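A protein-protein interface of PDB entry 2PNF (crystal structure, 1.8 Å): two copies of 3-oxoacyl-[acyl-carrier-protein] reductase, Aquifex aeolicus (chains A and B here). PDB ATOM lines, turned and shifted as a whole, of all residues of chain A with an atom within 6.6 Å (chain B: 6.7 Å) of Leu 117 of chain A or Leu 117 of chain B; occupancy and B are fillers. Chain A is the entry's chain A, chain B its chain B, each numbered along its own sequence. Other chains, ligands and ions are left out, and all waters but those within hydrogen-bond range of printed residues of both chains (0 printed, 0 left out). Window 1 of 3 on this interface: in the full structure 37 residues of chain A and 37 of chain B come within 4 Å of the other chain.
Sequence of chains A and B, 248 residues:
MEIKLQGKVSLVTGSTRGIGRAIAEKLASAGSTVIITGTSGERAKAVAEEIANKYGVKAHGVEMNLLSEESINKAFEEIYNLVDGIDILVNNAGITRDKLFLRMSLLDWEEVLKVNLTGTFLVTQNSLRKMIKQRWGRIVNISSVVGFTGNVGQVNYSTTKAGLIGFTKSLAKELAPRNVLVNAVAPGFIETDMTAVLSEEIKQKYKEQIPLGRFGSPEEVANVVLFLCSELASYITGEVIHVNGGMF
The side-chain hydroxyl (OG1) of Thr 159 of chain B sits close to the backbone NH (N) of Phe 167 of chain A, at 3.5 Å.
The indole nitrogen (NE1) of Trp 109 of chain A is in hydrogen-bond range of the side-chain hydroxyl (OG1) of Thr 118 of chain B (2.9 Å).
The side-chain hydroxyl (OG1) of Thr 118 of chain A lies within hydrogen-bond range of the indole nitrogen (NE1) of Trp 109 of chain B (3.0 Å).
Trp 109 of chain A touches Phe 167 of chain B, and with the chains exchanged Phe 167 of chain A touches Trp 109 of chain B.
Leu 113 of chain A touches Leu 117 of chain B, and with the chains exchanged Leu 117 of chain A touches Leu 113 of chain B.
Leu 113 of chain A touches Thr 118 of chain B, and with the chains exchanged Thr 118 of chain A touches Leu 113 of chain B.
Thr 159 of chain A touches Gly 163 of chain B, and with the chains exchanged Gly 163 of chain A touches Thr 159 of chain B.
Positions printed for both chains: 109, 112, 113, 114, 115, 116, 117, 118, 119, 120, 121, 122, 159, 160, 161, 162, 163, 164 and 167.
The backbone NH (N) of Thr 118 of chain A is in hydrogen-bond range of the backbone carbonyl oxygen (O) of Leu 113 of chain A (3.1 Å).
The backbone carbonyl oxygen of Leu 113 of chain B is in hydrogen-bond range of the backbone NH of Thr 118 of chain B, 3.2 Å away.
Of the 19 printed residues of chain B, 9 touch a printed residue of chain A.
Printed residues of chain B that touch a printed residue of chain A: Trp 109, Leu 113, Leu 117, Thr 118, Phe 121, Thr 159, Ala 162, Gly 163 and Phe 167.
Hydrophobic or aromatic side chains of chain A that line the printed part of chain B: Trp 109, Leu 113, Leu 117, Phe 121, Ala 162 and Phe 167.
Among the printed residues, no Asp or Glu carboxylate lies within 4 Å of a Lys or Arg side-chain nitrogen of the other chain.
Trp 109 of chain A touches Leu 117 of chain B.
Trp 109 of chain A touches Phe 167 of chain B.
Leu 113 of chain A touches Thr 118 of chain B (CD2 to OG1, 3.6 Å).
Trp 109 of chain B touches Leu 117 of chain A (CZ2 to O, 3.6 Å).
CB of Leu 117 of chain A touches CD2 of Leu 113 of chain B (3.8 Å).
CD1 of Leu 117 of chain B touches CD1 of Leu 117 of chain A, at 3.9 Å.
CG2 of Thr 159 of chain B touches CD2 of Leu 117 of chain A, at 3.9 Å.
CA of Gly 163 of chain B touches O of Thr 159 of chain A (3.3 Å).
CB of Phe 167 of chain B touches OG1 of Thr 159 of chain A (3.3 Å).
O of Ala 162 of chain A touches CB of Ala 162 of chain B, at 3.4 Å.
Leu 117 of chain A touches just these residues of chain B: Trp 109, Leu 113, Leu 117 and Thr 159.
Printed residues of chain B within 4 Å of Phe 121 of chain A: Trp 109 (3.4 Å).
Of the printed residues of chain B, Phe 167 of chain A touches Trp 109 and Thr 159.
Of chain A, only Trp 109 (3.6 Å), Leu 113 (3.8 Å) and Leu 117 (3.9 Å) come within 4 Å of Leu 117 of chain B.
Of the printed residues of chain A, Phe 121 of chain B touches Trp 109.
Of the printed residues of chain A, Thr 159 of chain B touches Leu 117 (3.9 Å), Gly 163 (3.4 Å) and Phe 167 (3.3 Å).
The nearest printed residue of chain B that does not touch Gly 163 of chain A is Ala 162 of chain B (4.1 Å).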
ATOM      1  N   TRP A 109      15.488   5.914 -22.071  1.00  0.00           N
ATOM      2  CA  TRP A 109      15.151   7.125 -22.825  1.00  0.00           C
ATOM      3  C   TRP A 109      13.653   7.371 -22.799  1.00  0.00           C
ATOM      4  O   TRP A 109      13.183   8.462 -22.409  1.00  0.00           O
ATOM      5  CB  TRP A 109      15.627   6.992 -24.284  1.00  0.00           C
ATOM      6  CG  TRP A 109      15.112   8.106 -25.220  1.00  0.00           C
ATOM      7  CD1 TRP A 109      13.971   8.088 -25.953  1.00  0.00           C
ATOM      8  CD2 TRP A 109      15.732   9.359 -25.473  1.00  0.00           C
ATOM      9  NE1 TRP A 109      13.835   9.265 -26.652  1.00  0.00           N
ATOM     10  CE2 TRP A 109      14.909  10.068 -26.368  1.00  0.00           C
ATOM     11  CE3 TRP A 109      16.913   9.963 -25.031  1.00  0.00           C
ATOM     12  CZ2 TRP A 109      15.231  11.346 -26.820  1.00  0.00           C
ATOM     13  CZ3 TRP A 109      17.223  11.214 -25.480  1.00  0.00           C
ATOM     14  CH2 TRP A 109      16.392  11.904 -26.366  1.00  0.00           C
ATOM     15  N   VAL A 112      11.784   8.512 -19.465  1.00  0.00           N
ATOM     16  CA  VAL A 112      12.076   9.904 -19.094  1.00  0.00           C
ATOM     17  C   VAL A 112      11.199  10.833 -19.931  1.00  0.00           C
ATOM     18  O   VAL A 112      10.614  11.783 -19.411  1.00  0.00           O
ATOM     19  CB  VAL A 112      13.584  10.227 -19.251  1.00  0.00           C
ATOM     20  CG1 VAL A 112      13.836  11.720 -19.017  1.00  0.00           C
ATOM     21  CG2 VAL A 112      14.362   9.417 -18.217  1.00  0.00           C
ATOM     22  N   LEU A 113      11.100  10.538 -21.228  1.00  0.00           N
ATOM     23  CA  LEU A 113      10.225  11.338 -22.075  1.00  0.00           C
ATOM     24  C   LEU A 113       8.758  11.143 -21.692  1.00  0.00           C
ATOM     25  O   LEU A 113       7.985  12.094 -21.691  1.00  0.00           O
ATOM     26  CB  LEU A 113      10.411  10.959 -23.547  1.00  0.00           C
ATOM     27  CG  LEU A 113      11.441  11.789 -24.319  1.00  0.00           C
ATOM     28  CD1 LEU A 113      12.853  11.521 -23.754  1.00  0.00           C
ATOM     29  CD2 LEU A 113      11.380  11.402 -25.800  1.00  0.00           C
ATOM     30  N   LYS A 114       8.378   9.930 -21.320  1.00  0.00           N
ATOM     31  CA  LYS A 114       6.965   9.626 -21.014  1.00  0.00           C
ATOM     32  C   LYS A 114       6.486  10.381 -19.794  1.00  0.00           C
ATOM     33  O   LYS A 114       5.394  10.943 -19.780  1.00  0.00           O
ATOM     34  CB  LYS A 114       6.787   8.096 -20.844  1.00  0.00           C
ATOM     35  CG  LYS A 114       5.366   7.631 -20.499  1.00  0.00           C
ATOM     36  CD  LYS A 114       4.326   7.951 -21.602  1.00  0.00           C
ATOM     37  CE  LYS A 114       2.935   7.408 -21.174  1.00  0.00           C
ATOM     38  NZ  LYS A 114       1.760   7.958 -21.931  1.00  0.00           N
ATOM     39  N   VAL A 115       7.316  10.419 -18.760  1.00  0.00           N
ATOM     40  CA  VAL A 115       6.930  11.124 -17.559  1.00  0.00           C
ATOM     41  C   VAL A 115       7.109  12.636 -17.671  1.00  0.00           C
ATOM     42  O   VAL A 115       6.180  13.399 -17.402  1.00  0.00           O
ATOM     43  CB  VAL A 115       7.769  10.648 -16.328  1.00  0.00           C
ATOM     44  CG1 VAL A 115       7.514  11.591 -15.104  1.00  0.00           C
ATOM     45  CG2 VAL A 115       7.400   9.167 -15.994  1.00  0.00           C
ATOM     46  N   ASN A 116       8.292  13.076 -18.106  1.00  0.00           N
ATOM     47  CA  ASN A 116       8.585  14.511 -18.110  1.00  0.00           C
ATOM     48  C   ASN A 116       7.888  15.361 -19.178  1.00  0.00           C
ATOM     49  O   ASN A 116       7.566  16.513 -18.930  1.00  0.00           O
ATOM     50  CB  ASN A 116      10.114  14.757 -18.152  1.00  0.00           C
ATOM     51  CG  ASN A 116      10.869  14.027 -17.024  1.00  0.00           C
ATOM     52  OD1 ASN A 116      10.257  13.387 -16.164  1.00  0.00           O
ATOM     53  ND2 ASN A 116      12.200  14.124 -17.031  1.00  0.00           N
ATOM     54  N   LEU A 117       7.660  14.796 -20.357  1.00  0.00           N
ATOM     55  CA  LEU A 117       6.992  15.530 -21.415  1.00  0.00           C
ATOM     56  C   LEU A 117       5.544  15.051 -21.558  1.00  0.00           C
ATOM     57  O   LEU A 117       4.637  15.846 -21.426  1.00  0.00           O
ATOM     58  CB  LEU A 117       7.747  15.341 -22.740  1.00  0.00           C
ATOM     59  CG  LEU A 117       9.171  15.940 -22.730  1.00  0.00           C
ATOM     60  CD1 LEU A 117       9.798  15.777 -24.143  1.00  0.00           C
ATOM     61  CD2 LEU A 117       9.112  17.396 -22.361  1.00  0.00           C
ATOM     62  N   THR A 118       5.330  13.764 -21.795  1.00  0.00           N
ATOM     63  CA  THR A 118       3.947  13.291 -22.005  1.00  0.00           C
ATOM     64  C   THR A 118       3.076  13.410 -20.754  1.00  0.00           C
ATOM     65  O   THR A 118       1.910  13.803 -20.824  1.00  0.00           O
ATOM     66  CB  THR A 118       3.968  11.880 -22.539  1.00  0.00           C
ATOM     67  OG1 THR A 118       4.675  11.888 -23.781  1.00  0.00           O
ATOM     68  CG2 THR A 118       2.526  11.360 -22.826  1.00  0.00           C
ATOM     69  N   GLY A 119       3.647  13.108 -19.602  1.00  0.00           N
ATOM     70  CA  GLY A 119       2.896  13.235 -18.350  1.00  0.00           C
ATOM     71  C   GLY A 119       2.515  14.680 -18.127  1.00  0.00           C
ATOM     72  O   GLY A 119       1.393  14.977 -17.731  1.00  0.00           O
ATOM     73  N   THR A 120       3.457  15.602 -18.366  1.00  0.00           N
ATOM     74  CA  THR A 120       3.183  17.016 -18.232  1.00  0.00           C
ATOM     75  C   THR A 120       2.105  17.428 -19.252  1.00  0.00           C
ATOM     76  O   THR A 120       1.231  18.209 -18.932  1.00  0.00           O
ATOM     77  CB  THR A 120       4.478  17.842 -18.470  1.00  0.00           C
ATOM     78  OG1 THR A 120       5.378  17.598 -17.389  1.00  0.00           O
ATOM     79  CG2 THR A 120       4.216  19.330 -18.605  1.00  0.00           C
ATOM     80  N   PHE A 121       2.203  16.927 -20.482  1.00  0.00           N
ATOM     81  CA  PHE A 121       1.168  17.238 -21.483  1.00  0.00           C
ATOM     82  C   PHE A 121      -0.232  16.833 -20.967  1.00  0.00           C
ATOM     83  O   PHE A 121      -1.173  17.636 -20.993  1.00  0.00           O
ATOM     84  CB  PHE A 121       1.475  16.477 -22.810  1.00  0.00           C
ATOM     85  CG  PHE A 121       0.328  16.424 -23.768  1.00  0.00           C
ATOM     86  CD1 PHE A 121       0.000  17.526 -24.541  1.00  0.00           C
ATOM     87  CD2 PHE A 121      -0.427  15.266 -23.894  1.00  0.00           C
ATOM     88  CE1 PHE A 121      -1.077  17.472 -25.445  1.00  0.00           C
ATOM     89  CE2 PHE A 121      -1.509  15.197 -24.789  1.00  0.00           C
ATOM     90  CZ  PHE A 121      -1.832  16.297 -25.563  1.00  0.00           C
ATOM     91  N   LEU A 122      -0.363  15.594 -20.525  1.00  0.00           N
ATOM     92  CA  LEU A 122      -1.670  15.064 -20.085  1.00  0.00           C
ATOM     93  C   LEU A 122      -2.202  15.741 -18.827  1.00  0.00           C
ATOM     94  O   LEU A 122      -3.384  16.088 -18.729  1.00  0.00           O
ATOM     95  CB  LEU A 122      -1.543  13.566 -19.835  1.00  0.00           C
ATOM     96  CG  LEU A 122      -1.637  12.757 -21.119  1.00  0.00           C
ATOM     97  CD1 LEU A 122      -1.238  11.275 -20.874  1.00  0.00           C
ATOM     98  CD2 LEU A 122      -3.116  12.863 -21.592  1.00  0.00           C
ATOM     99  N   THR A 159      17.155  16.641 -22.645  1.00  0.00           N
ATOM    100  CA  THR A 159      16.246  16.742 -23.773  1.00  0.00           C
ATOM    101  C   THR A 159      14.859  17.134 -23.244  1.00  0.00           C
ATOM    102  O   THR A 159      14.223  18.038 -23.778  1.00  0.00           O
ATOM    103  CB  THR A 159      16.162  15.388 -24.527  1.00  0.00           C
ATOM    104  OG1 THR A 159      17.414  15.136 -25.166  1.00  0.00           O
ATOM    105  CG2 THR A 159      15.055  15.410 -25.593  1.00  0.00           C
ATOM    106  N   THR A 160      14.381  16.461 -22.193  1.00  0.00           N
ATOM    107  CA  THR A 160      13.052  16.818 -21.678  1.00  0.00           C
ATOM    108  C   THR A 160      12.980  18.171 -20.977  1.00  0.00           C
ATOM    109  O   THR A 160      11.977  18.910 -21.098  1.00  0.00           O
ATOM    110  CB  THR A 160      12.466  15.721 -20.684  1.00  0.00           C
ATOM    111  OG1 THR A 160      13.237  15.692 -19.468  1.00  0.00           O
ATOM    112  CG2 THR A 160      12.483  14.302 -21.330  1.00  0.00           C
ATOM    113  N   LYS A 161      14.030  18.535 -20.234  1.00  0.00           N
ATOM    114  CA  LYS A 161      13.987  19.807 -19.544  1.00  0.00           C
ATOM    115  C   LYS A 161      14.067  20.979 -20.537  1.00  0.00           C
ATOM    116  O   LYS A 161      13.507  22.011 -20.265  1.00  0.00           O
ATOM    117  CB  LYS A 161      15.073  19.875 -18.456  1.00  0.00           C
ATOM    118  CG  LYS A 161      14.812  18.866 -17.303  1.00  0.00           C
ATOM    119  CD  LYS A 161      13.485  19.226 -16.622  1.00  0.00           C
ATOM    120  CE  LYS A 161      12.893  18.067 -15.807  1.00  0.00           C
ATOM    121  NZ  LYS A 161      11.595  18.413 -15.143  1.00  0.00           N
ATOM    122  N   ALA A 162      14.763  20.805 -21.674  1.00  0.00           N
ATOM    123  CA  ALA A 162      14.817  21.830 -22.701  1.00  0.00           C
ATOM    124  C   ALA A 162      13.459  21.786 -23.457  1.00  0.00           C
ATOM    125  O   ALA A 162      12.921  22.816 -23.842  1.00  0.00           O
ATOM    126  CB  ALA A 162      15.929  21.540 -23.688  1.00  0.00           C
ATOM    127  N   GLY A 163      12.945  20.578 -23.676  1.00  0.00           N
ATOM    128  CA  GLY A 163      11.655  20.448 -24.354  1.00  0.00           C
ATOM    129  C   GLY A 163      10.549  21.171 -23.616  1.00  0.00           C
ATOM    130  O   GLY A 163       9.643  21.759 -24.245  1.00  0.00           O
ATOM    131  N   LEU A 164      10.606  21.158 -22.293  1.00  0.00           N
ATOM    132  CA  LEU A 164       9.585  21.869 -21.510  1.00  0.00           C
ATOM    133  C   LEU A 164       9.556  23.372 -21.732  1.00  0.00           C
ATOM    134  O   LEU A 164       8.545  24.041 -21.452  1.00  0.00           O
ATOM    135  CB  LEU A 164       9.763  21.607 -20.028  1.00  0.00           C
ATOM    136  CG  LEU A 164       9.297  20.206 -19.683  1.00  0.00           C
ATOM    137  CD1 LEU A 164       9.822  19.820 -18.300  1.00  0.00           C
ATOM    138  CD2 LEU A 164       7.786  20.176 -19.723  1.00  0.00           C
ATOM    139  N   PHE A 167       7.560  23.780 -24.825  1.00  0.00           N
ATOM    140  CA  PHE A 167       6.193  23.536 -24.349  1.00  0.00           C
ATOM    141  C   PHE A 167       5.631  24.795 -23.675  1.00  0.00           C
ATOM    142  O   PHE A 167       4.527  25.251 -23.981  1.00  0.00           O
ATOM    143  CB  PHE A 167       6.224  22.374 -23.346  1.00  0.00           C
ATOM    144  CG  PHE A 167       4.879  22.024 -22.763  1.00  0.00           C
ATOM    145  CD1 PHE A 167       3.960  21.281 -23.510  1.00  0.00           C
ATOM    146  CD2 PHE A 167       4.541  22.424 -21.461  1.00  0.00           C
ATOM    147  CE1 PHE A 167       2.722  20.932 -22.962  1.00  0.00           C
ATOM    148  CE2 PHE A 167       3.294  22.079 -20.897  1.00  0.00           C
ATOM    149  CZ  PHE A 167       2.386  21.332 -21.646  1.00  0.00           C
ATOM    150  N   TRP B 109       0.242  14.060 -29.977  1.00  0.00           N
ATOM    151  CA  TRP B 109       1.425  14.371 -29.178  1.00  0.00           C
ATOM    152  C   TRP B 109       2.499  13.292 -29.222  1.00  0.00           C
ATOM    153  O   TRP B 109       3.647  13.569 -29.561  1.00  0.00           O
ATOM    154  CB  TRP B 109       1.011  14.628 -27.723  1.00  0.00           C
ATOM    155  CG  TRP B 109       2.188  14.798 -26.777  1.00  0.00           C
ATOM    156  CD1 TRP B 109       2.835  13.820 -26.083  1.00  0.00           C
ATOM    157  CD2 TRP B 109       2.815  16.035 -26.410  1.00  0.00           C
ATOM    158  NE1 TRP B 109       3.832  14.380 -25.301  1.00  0.00           N
ATOM    159  CE2 TRP B 109       3.835  15.733 -25.482  1.00  0.00           C
ATOM    160  CE3 TRP B 109       2.608  17.370 -26.776  1.00  0.00           C
ATOM    161  CZ2 TRP B 109       4.641  16.727 -24.912  1.00  0.00           C
ATOM    162  CZ3 TRP B 109       3.414  18.363 -26.211  1.00  0.00           C
ATOM    163  CH2 TRP B 109       4.413  18.028 -25.288  1.00  0.00           C
ATOM    164  N   VAL B 112       4.551  12.665 -32.617  1.00  0.00           N
ATOM    165  CA  VAL B 112       5.514  13.727 -32.882  1.00  0.00           C
ATOM    166  C   VAL B 112       6.744  13.541 -31.988  1.00  0.00           C
ATOM    167  O   VAL B 112       7.874  13.670 -32.447  1.00  0.00           O
ATOM    168  CB  VAL B 112       4.878  15.106 -32.661  1.00  0.00           C
ATOM    169  CG1 VAL B 112       5.961  16.211 -32.709  1.00  0.00           C
ATOM    170  CG2 VAL B 112       3.887  15.382 -33.783  1.00  0.00           C
ATOM    171  N   LEU B 113       6.546  13.236 -30.711  1.00  0.00           N
ATOM    172  CA  LEU B 113       7.726  12.986 -29.865  1.00  0.00           C
ATOM    173  C   LEU B 113       8.460  11.704 -30.257  1.00  0.00           C
ATOM    174  O   LEU B 113       9.693  11.664 -30.249  1.00  0.00           O
ATOM    175  CB  LEU B 113       7.307  12.865 -28.396  1.00  0.00           C
ATOM    176  CG  LEU B 113       7.292  14.159 -27.578  1.00  0.00           C
ATOM    177  CD1 LEU B 113       6.249  15.136 -28.100  1.00  0.00           C
ATOM    178  CD2 LEU B 113       7.048  13.794 -26.102  1.00  0.00           C
ATOM    179  N   LYS B 114       7.723  10.652 -30.627  1.00  0.00           N
ATOM    180  CA  LYS B 114       8.377   9.394 -30.952  1.00  0.00           C
ATOM    181  C   LYS B 114       9.247   9.479 -32.183  1.00  0.00           C
ATOM    182  O   LYS B 114      10.334   8.892 -32.236  1.00  0.00           O
ATOM    183  CB  LYS B 114       7.371   8.240 -31.096  1.00  0.00           C
ATOM    184  CG  LYS B 114       8.084   6.901 -31.286  1.00  0.00           C
ATOM    185  CD  LYS B 114       7.468   5.796 -30.450  1.00  0.00           C
ATOM    186  CE  LYS B 114       8.087   4.424 -30.783  1.00  0.00           C
ATOM    187  NZ  LYS B 114       9.590   4.402 -30.668  1.00  0.00           N
ATOM    188  N   VAL B 115       8.775  10.215 -33.177  1.00  0.00           N
ATOM    189  CA  VAL B 115       9.567  10.378 -34.386  1.00  0.00           C
ATOM    190  C   VAL B 115      10.688  11.387 -34.159  1.00  0.00           C
ATOM    191  O   VAL B 115      11.873  11.064 -34.364  1.00  0.00           O
ATOM    192  CB  VAL B 115       8.713  10.922 -35.574  1.00  0.00           C
ATOM    193  CG1 VAL B 115       9.605  11.286 -36.778  1.00  0.00           C
ATOM    194  CG2 VAL B 115       7.680   9.848 -36.004  1.00  0.00           C
ATOM    195  N   ASN B 116      10.320  12.595 -33.721  1.00  0.00           N
ATOM    196  CA  ASN B 116      11.304  13.697 -33.630  1.00  0.00           C
ATOM    197  C   ASN B 116      12.402  13.582 -32.563  1.00  0.00           C
ATOM    198  O   ASN B 116      13.541  14.025 -32.766  1.00  0.00           O
ATOM    199  CB  ASN B 116      10.568  15.041 -33.505  1.00  0.00           C
ATOM    200  CG  ASN B 116       9.617  15.339 -34.705  1.00  0.00           C
ATOM    201  OD1 ASN B 116       9.465  14.535 -35.624  1.00  0.00           O
ATOM    202  ND2 ASN B 116       8.980  16.508 -34.673  1.00  0.00           N
ATOM    203  N   LEU B 117      12.065  12.991 -31.435  1.00  0.00           N
ATOM    204  CA  LEU B 117      13.050  12.822 -30.366  1.00  0.00           C
ATOM    205  C   LEU B 117      13.544  11.387 -30.285  1.00  0.00           C
ATOM    206  O   LEU B 117      14.736  11.139 -30.360  1.00  0.00           O
ATOM    207  CB  LEU B 117      12.430  13.236 -29.005  1.00  0.00           C
ATOM    208  CG  LEU B 117      12.033  14.730 -28.942  1.00  0.00           C
ATOM    209  CD1 LEU B 117      11.491  15.080 -27.532  1.00  0.00           C
ATOM    210  CD2 LEU B 117      13.228  15.633 -29.277  1.00  0.00           C
ATOM    211  N   THR B 118      12.633  10.427 -30.136  1.00  0.00           N
ATOM    212  CA  THR B 118      13.053   9.040 -29.959  1.00  0.00           C
ATOM    213  C   THR B 118      13.671   8.456 -31.231  1.00  0.00           C
ATOM    214  O   THR B 118      14.688   7.756 -31.170  1.00  0.00           O
ATOM    215  CB  THR B 118      11.889   8.186 -29.436  1.00  0.00           C
ATOM    216  OG1 THR B 118      11.417   8.746 -28.201  1.00  0.00           O
ATOM    217  CG2 THR B 118      12.348   6.729 -29.157  1.00  0.00           C
ATOM    218  N   GLY B 119      13.103   8.786 -32.389  1.00  0.00           N
ATOM    219  CA  GLY B 119      13.706   8.304 -33.640  1.00  0.00           C
ATOM    220  C   GLY B 119      15.107   8.893 -33.802  1.00  0.00           C
ATOM    221  O   GLY B 119      16.055   8.211 -34.205  1.00  0.00           O
ATOM    222  N   THR B 120      15.238  10.188 -33.516  1.00  0.00           N
ATOM    223  CA  THR B 120      16.538  10.833 -33.589  1.00  0.00           C
ATOM    224  C   THR B 120      17.521  10.140 -32.614  1.00  0.00           C
ATOM    225  O   THR B 120      18.701   9.961 -32.921  1.00  0.00           O
ATOM    226  CB  THR B 120      16.397  12.286 -33.225  1.00  0.00           C
ATOM    227  OG1 THR B 120      15.526  12.911 -34.173  1.00  0.00           O
ATOM    228  CG2 THR B 120      17.739  12.994 -33.245  1.00  0.00           C
ATOM    229  N   PHE B 121      17.045   9.839 -31.407  1.00  0.00           N
ATOM    230  CA  PHE B 121      17.891   9.146 -30.395  1.00  0.00           C
ATOM    231  C   PHE B 121      18.451   7.831 -30.954  1.00  0.00           C
ATOM    232  O   PHE B 121      19.665   7.579 -30.956  1.00  0.00           O
ATOM    233  CB  PHE B 121      17.007   8.875 -29.149  1.00  0.00           C
ATOM    234  CG  PHE B 121      17.588   7.874 -28.169  1.00  0.00           C
ATOM    235  CD1 PHE B 121      18.699   8.184 -27.391  1.00  0.00           C
ATOM    236  CD2 PHE B 121      17.021   6.632 -28.041  1.00  0.00           C
ATOM    237  CE1 PHE B 121      19.235   7.246 -26.497  1.00  0.00           C
ATOM    238  CE2 PHE B 121      17.549   5.693 -27.156  1.00  0.00           C
ATOM    239  CZ  PHE B 121      18.662   6.009 -26.384  1.00  0.00           C
ATOM    240  N   LEU B 122      17.556   6.981 -31.442  1.00  0.00           N
ATOM    241  CA  LEU B 122      17.974   5.675 -31.982  1.00  0.00           C
ATOM    242  C   LEU B 122      18.893   5.777 -33.206  1.00  0.00           C
ATOM    243  O   LEU B 122      19.854   5.044 -33.313  1.00  0.00           O
ATOM    244  CB  LEU B 122      16.734   4.842 -32.324  1.00  0.00           C
ATOM    245  CG  LEU B 122      15.850   4.438 -31.128  1.00  0.00           C
ATOM    246  CD1 LEU B 122      14.556   3.805 -31.648  1.00  0.00           C
ATOM    247  CD2 LEU B 122      16.580   3.454 -30.227  1.00  0.00           C
ATOM    248  N   THR B 159       7.878  21.559 -28.648  1.00  0.00           N
ATOM    249  CA  THR B 159       8.490  20.815 -27.554  1.00  0.00           C
ATOM    250  C   THR B 159       9.637  19.970 -28.122  1.00  0.00           C
ATOM    251  O   THR B 159      10.758  19.923 -27.550  1.00  0.00           O
ATOM    252  CB  THR B 159       7.440  19.909 -26.852  1.00  0.00           C
ATOM    253  OG1 THR B 159       6.506  20.741 -26.153  1.00  0.00           O
ATOM    254  CG2 THR B 159       8.094  18.980 -25.807  1.00  0.00           C
ATOM    255  N   THR B 160       9.402  19.280 -29.242  1.00  0.00           N
ATOM    256  CA  THR B 160      10.478  18.459 -29.798  1.00  0.00           C
ATOM    257  C   THR B 160      11.647  19.302 -30.344  1.00  0.00           C
ATOM    258  O   THR B 160      12.817  18.930 -30.190  1.00  0.00           O
ATOM    259  CB  THR B 160       9.989  17.476 -30.915  1.00  0.00           C
ATOM    260  OG1 THR B 160       9.627  18.178 -32.103  1.00  0.00           O
ATOM    261  CG2 THR B 160       8.787  16.717 -30.396  1.00  0.00           C
ATOM    262  N   LYS B 161      11.364  20.435 -30.973  1.00  0.00           N
ATOM    263  CA  LYS B 161      12.479  21.209 -31.525  1.00  0.00           C
ATOM    264  C   LYS B 161      13.337  21.861 -30.423  1.00  0.00           C
ATOM    265  O   LYS B 161      14.554  22.017 -30.597  1.00  0.00           O
ATOM    266  CB  LYS B 161      11.984  22.233 -32.590  1.00  0.00           C
ATOM    267  CG  LYS B 161      11.428  21.482 -33.861  1.00  0.00           C
ATOM    268  CD  LYS B 161      12.383  20.340 -34.305  1.00  0.00           C
ATOM    269  CE  LYS B 161      11.864  19.601 -35.549  1.00  0.00           C
ATOM    270  NZ  LYS B 161      12.948  18.739 -36.173  1.00  0.00           N
ATOM    271  N   ALA B 162      12.681  22.213 -29.304  1.00  0.00           N
ATOM    272  CA  ALA B 162      13.387  22.764 -28.151  1.00  0.00           C
ATOM    273  C   ALA B 162      14.167  21.591 -27.512  1.00  0.00           C
ATOM    274  O   ALA B 162      15.308  21.756 -27.070  1.00  0.00           O
ATOM    275  CB  ALA B 162      12.415  23.313 -27.131  1.00  0.00           C
ATOM    276  N   GLY B 163      13.519  20.439 -27.425  1.00  0.00           N
ATOM    277  CA  GLY B 163      14.167  19.260 -26.853  1.00  0.00           C
ATOM    278  C   GLY B 163      15.444  18.900 -27.599  1.00  0.00           C
ATOM    279  O   GLY B 163      16.422  18.463 -26.993  1.00  0.00           O
ATOM    280  N   LEU B 164      15.443  19.036 -28.915  1.00  0.00           N
ATOM    281  CA  LEU B 164      16.666  18.704 -29.683  1.00  0.00           C
ATOM    282  C   LEU B 164      17.869  19.583 -29.293  1.00  0.00           C
ATOM    283  O   LEU B 164      19.030  19.182 -29.530  1.00  0.00           O
ATOM    284  CB  LEU B 164      16.409  18.847 -31.188  1.00  0.00           C
ATOM    285  CG  LEU B 164      15.511  17.741 -31.773  1.00  0.00           C
ATOM    286  CD1 LEU B 164      15.166  18.082 -33.238  1.00  0.00           C
ATOM    287  CD2 LEU B 164      16.197  16.411 -31.714  1.00  0.00           C
ATOM    288  N   PHE B 167      19.248  17.957 -26.207  1.00  0.00           N
ATOM    289  CA  PHE B 167      19.885  16.745 -26.747  1.00  0.00           C
ATOM    290  C   PHE B 167      21.285  17.088 -27.328  1.00  0.00           C
ATOM    291  O   PHE B 167      22.322  16.425 -27.039  1.00  0.00           O
ATOM    292  CB  PHE B 167      18.972  16.186 -27.875  1.00  0.00           C
ATOM    293  CG  PHE B 167      19.507  14.956 -28.562  1.00  0.00           C
ATOM    294  CD1 PHE B 167      19.311  13.701 -28.008  1.00  0.00           C
ATOM    295  CD2 PHE B 167      20.138  15.047 -29.806  1.00  0.00           C
ATOM    296  CE1 PHE B 167      19.725  12.537 -28.696  1.00  0.00           C
ATOM    297  CE2 PHE B 167      20.558  13.875 -30.512  1.00  0.00           C
ATOM    298  CZ  PHE B 167      20.345  12.632 -29.954  1.00  0.00           C
